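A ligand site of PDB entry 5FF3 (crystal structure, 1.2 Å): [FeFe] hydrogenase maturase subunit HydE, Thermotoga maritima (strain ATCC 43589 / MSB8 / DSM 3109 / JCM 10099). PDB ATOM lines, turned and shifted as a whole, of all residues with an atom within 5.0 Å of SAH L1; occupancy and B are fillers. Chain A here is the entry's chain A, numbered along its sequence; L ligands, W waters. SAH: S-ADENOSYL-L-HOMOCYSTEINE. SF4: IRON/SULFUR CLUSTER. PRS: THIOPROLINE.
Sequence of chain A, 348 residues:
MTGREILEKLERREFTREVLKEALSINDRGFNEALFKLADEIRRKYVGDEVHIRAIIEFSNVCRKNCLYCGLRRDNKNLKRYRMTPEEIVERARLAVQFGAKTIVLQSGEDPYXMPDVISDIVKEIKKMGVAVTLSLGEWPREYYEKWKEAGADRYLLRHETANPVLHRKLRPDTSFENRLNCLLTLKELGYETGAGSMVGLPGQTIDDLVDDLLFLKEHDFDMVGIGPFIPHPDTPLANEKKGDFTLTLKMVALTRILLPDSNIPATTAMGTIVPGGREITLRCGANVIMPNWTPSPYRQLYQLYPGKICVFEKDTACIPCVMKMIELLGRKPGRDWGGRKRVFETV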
ATOM      1  N   TYR A  69      14.893 -30.925 -21.562  1.00  0.00           N
ATOM      2  CA  TYR A  69      15.582 -31.616 -22.671  1.00  0.00           C
ATOM      3  C   TYR A  69      16.696 -30.820 -23.291  1.00  0.00           C
ATOM      4  O   TYR A  69      17.542 -31.386 -24.040  1.00  0.00           O
ATOM      5  CB  TYR A  69      14.588 -32.055 -23.772  1.00  0.00           C
ATOM      6  CG  TYR A  69      13.604 -31.004 -24.146  1.00  0.00           C
ATOM      7  CD1 TYR A  69      13.936 -29.983 -25.035  1.00  0.00           C
ATOM      8  CD2 TYR A  69      12.269 -30.964 -23.649  1.00  0.00           C
ATOM      9  CE1 TYR A  69      13.053 -28.996 -25.364  1.00  0.00           C
ATOM     10  CE2 TYR A  69      11.386 -30.002 -23.991  1.00  0.00           C
ATOM     11  CZ  TYR A  69      11.763 -28.993 -24.858  1.00  0.00           C
ATOM     12  OH  TYR A  69      10.844 -28.033 -25.155  1.00  0.00           O
ATOM     13  N   CYS A  70      16.742 -29.489 -23.071  1.00  0.00           N
ATOM     14  CA  CYS A  70      17.468 -28.596 -23.965  1.00  0.00           C
ATOM     15  C   CYS A  70      18.794 -28.184 -23.378  1.00  0.00           C
ATOM     16  O   CYS A  70      18.840 -27.653 -22.216  1.00  0.00           O
ATOM     17  CB  CYS A  70      16.662 -27.367 -24.201  1.00  0.00           C
ATOM     18  SG  CYS A  70      17.435 -26.225 -25.403  1.00  0.00           S
ATOM     19  N   GLN A 107      16.880 -17.981 -35.496  1.00  0.00           N
ATOM     20  CA  GLN A 107      16.510 -18.813 -34.339  1.00  0.00           C
ATOM     21  C   GLN A 107      17.418 -18.453 -33.171  1.00  0.00           C
ATOM     22  O   GLN A 107      18.603 -18.143 -33.332  1.00  0.00           O
ATOM     23  CB  GLN A 107      16.608 -20.329 -34.641  1.00  0.00           C
ATOM     24  CG  GLN A 107      16.024 -21.172 -33.500  1.00  0.00           C
ATOM     25  CD  GLN A 107      16.074 -22.625 -33.831  1.00  0.00           C
ATOM     26  OE1 GLN A 107      17.122 -23.283 -33.632  1.00  0.00           O
ATOM     27  NE2 GLN A 107      14.984 -23.201 -34.261  1.00  0.00           N
ATOM     28  N   SER A 108      16.833 -18.514 -31.963  1.00  0.00           N
ATOM     29  CA  SER A 108      17.621 -18.254 -30.769  1.00  0.00           C
ATOM     30  C   SER A 108      16.943 -18.931 -29.567  1.00  0.00           C
ATOM     31  O   SER A 108      15.795 -19.374 -29.616  1.00  0.00           O
ATOM     32  CB  SER A 108      17.679 -16.744 -30.492  1.00  0.00           C
ATOM     33  OG  SER A 108      16.402 -16.169 -30.293  1.00  0.00           O
ATOM     34  N   GLY A 109      17.716 -18.990 -28.469  1.00  0.00           N
ATOM     35  CA  GLY A 109      17.048 -19.157 -27.177  1.00  0.00           C
ATOM     36  C   GLY A 109      16.108 -17.999 -26.961  1.00  0.00           C
ATOM     37  O   GLY A 109      16.112 -16.973 -27.672  1.00  0.00           O
ATOM     38  N   GLU A 110      15.308 -18.115 -25.909  1.00  0.00           N
ATOM     39  CA  GLU A 110      14.427 -16.993 -25.513  1.00  0.00           C
ATOM     40  C   GLU A 110      15.281 -15.947 -24.802  1.00  0.00           C
ATOM     41  O   GLU A 110      15.346 -15.904 -23.537  1.00  0.00           O
ATOM     42  CB  GLU A 110      13.261 -17.449 -24.649  1.00  0.00           C
ATOM     43  CG  GLU A 110      12.238 -18.246 -25.434  1.00  0.00           C
ATOM     44  CD  GLU A 110      10.897 -18.410 -24.689  1.00  0.00           C
ATOM     45  OE1 GLU A 110      10.728 -17.790 -23.622  1.00  0.00           O
ATOM     46  OE2 GLU A 110      10.051 -19.176 -25.177  1.00  0.00           O
ATOM     47  N   SER A 136      12.137 -17.970 -35.277  1.00  0.00           N
ATOM     48  CA  SER A 136      11.948 -19.076 -34.360  1.00  0.00           C
ATOM     49  C   SER A 136      12.570 -18.679 -33.027  1.00  0.00           C
ATOM     50  O   SER A 136      13.673 -19.046 -32.679  1.00  0.00           O
ATOM     51  CB  SER A 136      12.616 -20.314 -34.947  1.00  0.00           C
ATOM     52  OG  SER A 136      12.447 -21.480 -34.127  1.00  0.00           O
ATOM     53  N   LEU A 137      11.817 -17.841 -32.267  1.00  0.00           N
ATOM     54  CA  LEU A 137      12.324 -17.139 -31.088  1.00  0.00           C
ATOM     55  C   LEU A 137      11.633 -17.586 -29.805  1.00  0.00           C
ATOM     56  O   LEU A 137      11.926 -17.046 -28.736  1.00  0.00           O
ATOM     57  CB  LEU A 137      12.215 -15.626 -31.255  1.00  0.00           C
ATOM     58  CG  LEU A 137      12.730 -15.074 -32.529  1.00  0.00           C
ATOM     59  CD1 LEU A 137      12.503 -13.558 -32.604  1.00  0.00           C
ATOM     60  CD2 LEU A 137      14.198 -15.437 -32.839  1.00  0.00           C
ATOM     61  N   GLY A 138      10.698 -18.549 -29.890  1.00  0.00           N
ATOM     62  CA  GLY A 138       9.959 -18.988 -28.693  1.00  0.00           C
ATOM     63  C   GLY A 138       8.684 -18.207 -28.443  1.00  0.00           C
ATOM     64  O   GLY A 138       8.067 -17.656 -29.369  1.00  0.00           O
ATOM     65  N   LEU A 157       8.263 -20.404 -36.635  1.00  0.00           N
ATOM     66  CA  LEU A 157       8.336 -21.780 -36.195  1.00  0.00           C
ATOM     67  C   LEU A 157       8.222 -21.884 -34.692  1.00  0.00           C
ATOM     68  O   LEU A 157       9.001 -21.240 -33.976  1.00  0.00           O
ATOM     69  CB  LEU A 157       9.683 -22.403 -36.610  1.00  0.00           C
ATOM     70  CG  LEU A 157      10.109 -22.254 -38.050  1.00  0.00           C
ATOM     71  CD1 LEU A 157      11.480 -22.839 -38.243  1.00  0.00           C
ATOM     72  CD2 LEU A 157       9.070 -22.828 -39.015  1.00  0.00           C
ATOM     73  N   LEU A 158       7.264 -22.633 -34.235  1.00  0.00           N
ATOM     74  CA  LEU A 158       7.052 -22.812 -32.775  1.00  0.00           C
ATOM     75  C   LEU A 158       6.559 -24.222 -32.585  1.00  0.00           C
ATOM     76  O   LEU A 158       5.350 -24.491 -32.541  1.00  0.00           O
ATOM     77  CB  LEU A 158       6.113 -21.757 -32.206  1.00  0.00           C
ATOM     78  CG  LEU A 158       6.075 -21.685 -30.708  1.00  0.00           C
ATOM     79  CD1 LEU A 158       7.341 -21.056 -30.164  1.00  0.00           C
ATOM     80  CD2 LEU A 158       4.830 -20.885 -30.232  1.00  0.00           C
ATOM     81  N   ARG A 159       7.483 -25.155 -32.508  1.00  0.00           N
ATOM     82  CA  ARG A 159       7.062 -26.516 -32.357  1.00  0.00           C
ATOM     83  C   ARG A 159       6.177 -26.693 -31.114  1.00  0.00           C
ATOM     84  O   ARG A 159       6.449 -26.113 -30.073  1.00  0.00           O
ATOM     85  CB  ARG A 159       8.223 -27.426 -32.197  1.00  0.00           C
ATOM     86  CG  ARG A 159       9.028 -27.553 -33.467  1.00  0.00           C
ATOM     87  CD  ARG A 159      10.106 -28.569 -33.223  1.00  0.00           C
ATOM     88  NE  ARG A 159      10.974 -28.731 -34.358  1.00  0.00           N
ATOM     89  CZ  ARG A 159      11.876 -29.692 -34.463  1.00  0.00           C
ATOM     90  NH1 ARG A 159      12.091 -30.456 -33.403  1.00  0.00           N
ATOM     91  NH2 ARG A 159      12.578 -29.861 -35.575  1.00  0.00           N
ATOM     92  N   GLU A 161       5.993 -29.408 -29.491  1.00  0.00           N
ATOM     93  CA  GLU A 161       6.847 -30.261 -28.681  1.00  0.00           C
ATOM     94  C   GLU A 161       6.231 -31.625 -28.302  1.00  0.00           C
ATOM     95  O   GLU A 161       6.802 -32.666 -28.594  1.00  0.00           O
ATOM     96  CB  GLU A 161       7.384 -29.541 -27.419  1.00  0.00           C
ATOM     97  CG  GLU A 161       7.969 -28.153 -27.697  1.00  0.00           C
ATOM     98  CD  GLU A 161       9.184 -28.096 -28.629  1.00  0.00           C
ATOM     99  OE1 GLU A 161       9.574 -29.140 -29.183  1.00  0.00           O
ATOM    100  OE2 GLU A 161       9.690 -26.974 -28.771  1.00  0.00           O
ATOM    101  N   ARG A 172       8.605 -28.647 -19.635  1.00  0.00           N
ATOM    102  CA  ARG A 172       8.727 -27.191 -19.922  1.00  0.00           C
ATOM    103  C   ARG A 172       8.121 -26.395 -18.764  1.00  0.00           C
ATOM    104  O   ARG A 172       7.022 -25.861 -18.861  1.00  0.00           O
ATOM    105  CB  ARG A 172       8.101 -26.893 -21.278  1.00  0.00           C
ATOM    106  CG  ARG A 172       8.579 -27.843 -22.354  1.00  0.00           C
ATOM    107  CD  ARG A 172       8.108 -27.425 -23.745  1.00  0.00           C
ATOM    108  NE  ARG A 172       8.769 -26.167 -24.135  1.00  0.00           N
ATOM    109  CZ  ARG A 172       8.185 -24.989 -24.259  1.00  0.00           C
ATOM    110  NH1 ARG A 172       6.916 -24.831 -24.241  1.00  0.00           N
ATOM    111  NH2 ARG A 172       8.975 -23.906 -24.378  1.00  0.00           N
ATOM    112  N   ARG A 180       1.537 -22.580 -25.281  1.00  0.00           N
ATOM    113  CA  ARG A 180       2.156 -22.884 -26.575  1.00  0.00           C
ATOM    114  C   ARG A 180       1.147 -22.827 -27.708  1.00  0.00           C
ATOM    115  O   ARG A 180       1.379 -22.232 -28.752  1.00  0.00           O
ATOM    116  CB  ARG A 180       2.833 -24.234 -26.489  1.00  0.00           C
ATOM    117  CG  ARG A 180       3.869 -24.550 -27.602  1.00  0.00           C
ATOM    118  CD  ARG A 180       5.133 -23.850 -27.269  1.00  0.00           C
ATOM    119  NE  ARG A 180       6.249 -24.283 -28.115  1.00  0.00           N
ATOM    120  CZ  ARG A 180       7.475 -23.773 -28.079  1.00  0.00           C
ATOM    121  NH1 ARG A 180       7.770 -22.774 -27.221  1.00  0.00           N
ATOM    122  NH2 ARG A 180       8.409 -24.167 -28.914  1.00  0.00           N
ATOM    123  N   MET A 199       8.958 -33.494 -30.815  1.00  0.00           N
ATOM    124  CA  MET A 199      10.030 -34.440 -30.681  1.00  0.00           C
ATOM    125  C   MET A 199       9.440 -35.836 -30.476  1.00  0.00           C
ATOM    126  O   MET A 199       8.309 -36.008 -29.983  1.00  0.00           O
ATOM    127  CB  MET A 199      10.920 -34.115 -29.497  1.00  0.00           C
ATOM    128  CG  MET A 199      11.829 -32.864 -29.766  1.00  0.00           C
ATOM    129  SD  MET A 199      12.762 -32.365 -28.312  1.00  0.00           S
ATOM    130  CE  MET A 199      11.488 -31.526 -27.388  1.00  0.00           C
ATOM    131  N   PRO A 229      13.907 -36.508 -33.591  1.00  0.00           N
ATOM    132  CA  PRO A 229      14.045 -37.295 -32.378  1.00  0.00           C
ATOM    133  C   PRO A 229      14.523 -36.427 -31.280  1.00  0.00           C
ATOM    134  O   PRO A 229      15.204 -35.442 -31.430  1.00  0.00           O
ATOM    135  CB  PRO A 229      15.176 -38.277 -32.725  1.00  0.00           C
ATOM    136  CG  PRO A 229      16.073 -37.482 -33.640  1.00  0.00           C
ATOM    137  CD  PRO A 229      15.075 -36.715 -34.475  1.00  0.00           C
ATOM    138  N   PHE A 230      14.140 -36.839 -30.061  1.00  0.00           N
ATOM    139  CA  PHE A 230      14.786 -36.349 -28.833  1.00  0.00           C
ATOM    140  C   PHE A 230      16.192 -36.865 -28.730  1.00  0.00           C
ATOM    141  O   PHE A 230      16.423 -38.061 -28.918  1.00  0.00           O
ATOM    142  CB  PHE A 230      13.974 -36.800 -27.576  1.00  0.00           C
ATOM    143  CG  PHE A 230      14.742 -36.695 -26.279  1.00  0.00           C
ATOM    144  CD1 PHE A 230      15.147 -35.472 -25.784  1.00  0.00           C
ATOM    145  CD2 PHE A 230      15.091 -37.858 -25.601  1.00  0.00           C
ATOM    146  CE1 PHE A 230      15.902 -35.409 -24.601  1.00  0.00           C
ATOM    147  CE2 PHE A 230      15.843 -37.774 -24.413  1.00  0.00           C
ATOM    148  CZ  PHE A 230      16.208 -36.557 -23.936  1.00  0.00           C
ATOM    149  N   ILE A 231      17.153 -36.017 -28.482  1.00  0.00           N
ATOM    150  CA  ILE A 231      18.551 -36.423 -28.358  1.00  0.00           C
ATOM    151  C   ILE A 231      19.051 -35.953 -26.956  1.00  0.00           C
ATOM    152  O   ILE A 231      19.132 -34.749 -26.726  1.00  0.00           O
ATOM    153  CB  ILE A 231      19.453 -35.858 -29.484  1.00  0.00           C
ATOM    154  CG1 ILE A 231      18.930 -36.349 -30.849  1.00  0.00           C
ATOM    155  CG2 ILE A 231      20.913 -36.250 -29.252  1.00  0.00           C
ATOM    156  CD1 ILE A 231      19.595 -35.640 -32.037  1.00  0.00           C
ATOM    157  N   PRO A 232      19.387 -36.891 -26.030  1.00  0.00           N
ATOM    158  CA  PRO A 232      19.731 -36.436 -24.695  1.00  0.00           C
ATOM    159  C   PRO A 232      20.984 -35.617 -24.673  1.00  0.00           C
ATOM    160  O   PRO A 232      21.988 -35.891 -25.372  1.00  0.00           O
ATOM    161  CB  PRO A 232      19.879 -37.790 -23.944  1.00  0.00           C
ATOM    162  CG  PRO A 232      20.351 -38.751 -25.015  1.00  0.00           C
ATOM    163  CD  PRO A 232      19.574 -38.345 -26.239  1.00  0.00           C
ATOM    164  N   HIS A 233      21.013 -34.567 -23.814  1.00  0.00           N
ATOM    165  CA  HIS A 233      22.101 -33.653 -23.650  1.00  0.00           C
ATOM    166  C   HIS A 233      22.711 -33.878 -22.236  1.00  0.00           C
ATOM    167  O   HIS A 233      21.986 -33.877 -21.258  1.00  0.00           O
ATOM    168  CB  HIS A 233      21.677 -32.181 -23.858  1.00  0.00           C
ATOM    169  CG  HIS A 233      22.800 -31.218 -23.909  1.00  0.00           C
ATOM    170  ND1 HIS A 233      23.657 -31.009 -22.852  1.00  0.00           N
ATOM    171  CD2 HIS A 233      23.239 -30.432 -24.897  1.00  0.00           C
ATOM    172  CE1 HIS A 233      24.554 -30.091 -23.192  1.00  0.00           C
ATOM    173  NE2 HIS A 233      24.324 -29.742 -24.437  1.00  0.00           N
ATOM    174  N   ALA A 270      18.497 -32.868 -36.556  1.00  0.00           N
ATOM    175  CA  ALA A 270      18.494 -33.944 -35.542  1.00  0.00           C
ATOM    176  C   ALA A 270      18.377 -35.297 -36.228  1.00  0.00           C
ATOM    177  O   ALA A 270      19.008 -36.264 -35.772  1.00  0.00           O
ATOM    178  CB  ALA A 270      17.394 -33.717 -34.533  1.00  0.00           C
ATOM    179  N   TYR A 303      25.914 -23.530 -30.029  1.00  0.00           N
ATOM    180  CA  TYR A 303      24.466 -23.631 -30.121  1.00  0.00           C
ATOM    181  C   TYR A 303      24.078 -25.053 -30.092  1.00  0.00           C
ATOM    182  O   TYR A 303      23.939 -25.697 -31.142  1.00  0.00           O
ATOM    183  CB  TYR A 303      23.931 -22.904 -31.342  1.00  0.00           C
ATOM    184  CG  TYR A 303      22.417 -22.718 -31.312  1.00  0.00           C
ATOM    185  CD1 TYR A 303      21.844 -21.586 -30.664  1.00  0.00           C
ATOM    186  CD2 TYR A 303      21.572 -23.635 -31.892  1.00  0.00           C
ATOM    187  CE1 TYR A 303      20.496 -21.380 -30.648  1.00  0.00           C
ATOM    188  CE2 TYR A 303      20.236 -23.431 -31.902  1.00  0.00           C
ATOM    189  CZ  TYR A 303      19.685 -22.333 -31.249  1.00  0.00           C
ATOM    190  OH  TYR A 303      18.294 -22.089 -31.288  1.00  0.00           O
ATOM    191  N   LEU A 305      21.520 -27.404 -28.656  1.00  0.00           N
ATOM    192  CA  LEU A 305      20.258 -27.901 -28.111  1.00  0.00           C
ATOM    193  C   LEU A 305      20.477 -29.306 -27.685  1.00  0.00           C
ATOM    194  O   LEU A 305      19.981 -29.750 -26.630  1.00  0.00           O
ATOM    195  CB  LEU A 305      19.177 -27.819 -29.218  1.00  0.00           C
ATOM    196  CG  LEU A 305      18.939 -26.420 -29.834  1.00  0.00           C
ATOM    197  CD1 LEU A 305      18.038 -26.585 -31.058  1.00  0.00           C
ATOM    198  CD2 LEU A 305      18.335 -25.480 -28.803  1.00  0.00           C
ATOM    199  N   TYR A 306      21.185 -30.085 -28.495  1.00  0.00           N
ATOM    200  CA  TYR A 306      21.589 -31.440 -28.266  1.00  0.00           C
ATOM    201  C   TYR A 306      23.010 -31.570 -28.716  1.00  0.00           C
ATOM    202  O   TYR A 306      23.518 -30.728 -29.468  1.00  0.00           O
ATOM    203  CB  TYR A 306      20.711 -32.490 -28.956  1.00  0.00           C
ATOM    204  CG  TYR A 306      20.502 -32.198 -30.432  1.00  0.00           C
ATOM    205  CD1 TYR A 306      21.472 -32.607 -31.383  1.00  0.00           C
ATOM    206  CD2 TYR A 306      19.458 -31.465 -30.877  1.00  0.00           C
ATOM    207  CE1 TYR A 306      21.322 -32.332 -32.695  1.00  0.00           C
ATOM    208  CE2 TYR A 306      19.290 -31.130 -32.226  1.00  0.00           C
ATOM    209  CZ  TYR A 306      20.254 -31.615 -33.127  1.00  0.00           C
ATOM    210  OH  TYR A 306      20.173 -31.314 -34.470  1.00  0.00           O
HETATM  211  N   SAH L   1      13.720 -21.421 -28.083  1.00  0.00           N
HETATM  212  CA  SAH L   1      12.937 -21.640 -29.293  1.00  0.00           C
HETATM  213  CB  SAH L   1      13.861 -22.004 -30.497  1.00  0.00           C
HETATM  214  CG  SAH L   1      15.031 -22.935 -30.301  1.00  0.00           C
HETATM  215  SD  SAH L   1      14.725 -24.523 -29.614  1.00  0.00           S
HETATM  216  C   SAH L   1      11.891 -22.620 -29.006  1.00  0.00           C
HETATM  217  O   SAH L   1      10.935 -22.684 -29.806  1.00  0.00           O
HETATM  218  OXT SAH L   1      11.974 -23.286 -27.937  1.00  0.00           O
HETATM  219  C5' SAH L   1      14.205 -25.326 -31.217  1.00  0.00           C
HETATM  220  C4' SAH L   1      13.690 -26.792 -31.144  1.00  0.00           C
HETATM  221  O4' SAH L   1      14.778 -27.729 -30.853  1.00  0.00           O
HETATM  222  C3' SAH L   1      12.716 -27.103 -30.125  1.00  0.00           C
HETATM  223  O3' SAH L   1      11.418 -26.709 -30.586  1.00  0.00           O
HETATM  224  C2' SAH L   1      12.841 -28.607 -29.801  1.00  0.00           C
HETATM  225  O2' SAH L   1      11.899 -29.423 -30.506  1.00  0.00           O
HETATM  226  C1' SAH L   1      14.221 -28.963 -30.327  1.00  0.00           C
HETATM  227  N9  SAH L   1      15.175 -29.448 -29.375  1.00  0.00           N
HETATM  228  C8  SAH L   1      15.521 -28.867 -28.204  1.00  0.00           C
HETATM  229  N7  SAH L   1      16.270 -29.638 -27.443  1.00  0.00           N
HETATM  230  C5  SAH L   1      16.367 -30.820 -28.122  1.00  0.00           C
HETATM  231  C6  SAH L   1      16.999 -32.071 -27.868  1.00  0.00           C
HETATM  232  N6  SAH L   1      17.618 -32.365 -26.720  1.00  0.00           N
HETATM  233  N1  SAH L   1      16.870 -33.052 -28.796  1.00  0.00           N
HETATM  234  C2  SAH L   1      16.225 -32.839 -29.975  1.00  0.00           C
HETATM  235  N3  SAH L   1      15.650 -31.708 -30.273  1.00  0.00           N
HETATM  236  C4  SAH L   1      15.679 -30.706 -29.386  1.00  0.00           C
HETATM  237 FE1  SF4 L   2      15.841 -24.600 -25.292  1.00  0.00          FE
HETATM  238 FE2  SF4 L   2      15.136 -22.196 -24.326  1.00  0.00          FE
HETATM  239 FE3  SF4 L   2      13.396 -24.275 -24.132  1.00  0.00          FE
HETATM  240 FE4  SF4 L   2      13.868 -23.129 -26.750  1.00  0.00          FE
HETATM  241  S1  SF4 L   2      12.858 -22.183 -24.766  1.00  0.00           S
HETATM  242  S2  SF4 L   2      13.844 -25.417 -26.093  1.00  0.00           S
HETATM  243  S3  SF4 L   2      16.196 -22.646 -26.294  1.00  0.00           S
HETATM  244  S4  SF4 L   2      15.426 -24.056 -23.064  1.00  0.00           S
HETATM  245  N   PRS L   3      15.761 -28.106 -36.534  1.00  0.00           N
HETATM  246  CD  PRS L   3      14.953 -26.844 -36.340  1.00  0.00           C
HETATM  247  CA  PRS L   3      16.834 -28.144 -35.506  1.00  0.00           C
HETATM  248  CB  PRS L   3      16.078 -27.738 -34.269  1.00  0.00           C
HETATM  249  SG  PRS L   3      14.537 -26.707 -34.613  1.00  0.00           S
HETATM  250  C   PRS L   3      17.525 -29.468 -35.422  1.00  0.00           C
HETATM  251  O   PRS L   3      17.026 -30.469 -35.797  1.00  0.00           O
HETATM  252  OXT PRS L   3      18.694 -29.333 -34.956  1.00  0.00           O
HETATM  253  O   HOH W   1      10.116 -21.578 -26.416  1.00  0.00           O
HETATM  254  O   HOH W   2      14.382 -32.735 -32.589  1.00  0.00           O
HETATM  255  O   HOH W   3      10.347 -24.571 -31.837  1.00  0.00           O
HETATM  256  O   HOH W   4      10.672 -25.734 -26.514  1.00  0.00           O
HETATM  257  O   HOH W   5      10.655 -20.848 -31.889  1.00  0.00           O
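Water W3 lies within hydrogen-bond range of O3' of SAH L1 (2.7 Å) and N of Arg 159 (3.0 Å). Water W5 lies within hydrogen-bond range of O of Leu 157 (2.7 Å), O of SAH L1 (2.8 Å), OG of Ser 136 (2.9 Å), N of Gly 138 (3.0 Å) and N of Leu 137 (3.2 Å). Water W2 lies within hydrogen-bond range of a nitrogen (N3) of SAH L1, the backbone carbonyl oxygen (O) of Pro 229 and the guanidinium group (NH1) of Arg 159. Water W1 lies within hydrogen-bond range of OE2 of Glu 110 (2.7 Å), NH1 of Arg 180 (2.8 Å), S1 of SF4 L2 (3.3 Å) and NH2 of Arg 172 (3.3 Å). Water W4 lies within hydrogen-bond range of the side-chain hydroxyl of Tyr 69 (2.7 Å), the side-chain carboxylate of Glu 161 (2.8 Å), the guanidinium group of Arg 172 (3.1 Å) and a sulfur (S2) of SF4 L2 (3.2 Å).
An oxygen (O) of PRS L3 sits at hydrogen-bond distance from the backbone NH (N) of Ala 270, at 2.9 Å. O3' of SAH L1 sits at hydrogen-bond distance from OE2 of Glu 161, 2.5 Å away. NH2 of Arg 180 lies within salt-bridge range of O of SAH L1 (3.1 Å). A sulfur (SG) of PRS L3 lies close to the side-chain amide nitrogen of Gln 107. The side-chain sulfur (SG) of Cys 70 is bound to an iron atom (FE1) of SF4 L2 (2.3 Å). The side-chain sulfur of Met 199 lies close to an oxygen (O2') of SAH L1 (3.8 Å). An oxygen (O2') of SAH L1 sits at hydrogen-bond distance from the guanidinium group (NH1) of Arg 159 (3.1 Å). N6 of SAH L1 sits at hydrogen-bond distance from O of Tyr 69 (2.9 Å). The backbone carbonyl oxygen of Ser 108 sits close to a nitrogen (N) of SAH L1 (3.3 Å). OXT of PRS L3 is in hydrogen-bond range of OH of Tyr 306 (2.5 Å). N6 of SAH L1 is in hydrogen-bond range of O of Ile 231 (2.8 Å). The backbone NH (N) of Ile 231 is in hydrogen-bond range of a nitrogen (N1) of SAH L1.
A nitrogen (N) of SAH L1 is bound to an iron atom (FE4) of SF4 L2 (2.2 Å).
N of Ser 108 sits at hydrogen-bond distance from O of Ser 136 (3.3 Å). The side-chain amide nitrogen (NE2) of Gln 107 lies within hydrogen-bond range of the side-chain hydroxyl (OG) of Ser 136, at 3.1 Å. The guanidinium group of Arg 180 sits at hydrogen-bond distance from the backbone carbonyl oxygen of Arg 159 (2.7 Å). The side-chain hydroxyl of Tyr 303 lies within hydrogen-bond range of the side-chain amide oxygen of Gln 107 (2.9 Å). The backbone carbonyl oxygen of Glu 161 sits at hydrogen-bond distance from the backbone NH of Met 199 (3.2 Å). OE2 of Glu 161 lies within salt-bridge range of NH2 of Arg 180, at 3.1 Å. OH of Tyr 306 lies within hydrogen-bond range of N of Ala 270 (3.1 Å). The side-chain hydroxyl (OH) of Tyr 69 is in hydrogen-bond range of the guanidinium group (NE) of Arg 172, 3.0 Å away.
CA of Cys 70 touches N7 of SAH L1 (3.8 Å). Gln 107 touches SAH L1 (CD to CG, 3.7 Å). Ser 136 touches SAH L1. N of Gly 138 touches CA of SAH L1, 3.9 Å away. CD1 of Leu 158 touches O of SAH L1 (3.96 Å). Pro 229 touches SAH L1. Phe 230 touches SAH L1. Tyr 303 touches SAH L1 (OH to CG, 3.5 Å). Leu 305 touches SAH L1. Tyr 306 touches SAH L1 (CD2 to C2, 3.6 Å). The nearest printed residue that does not touch SAH L1 is Gly 109 (4.1 Å).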
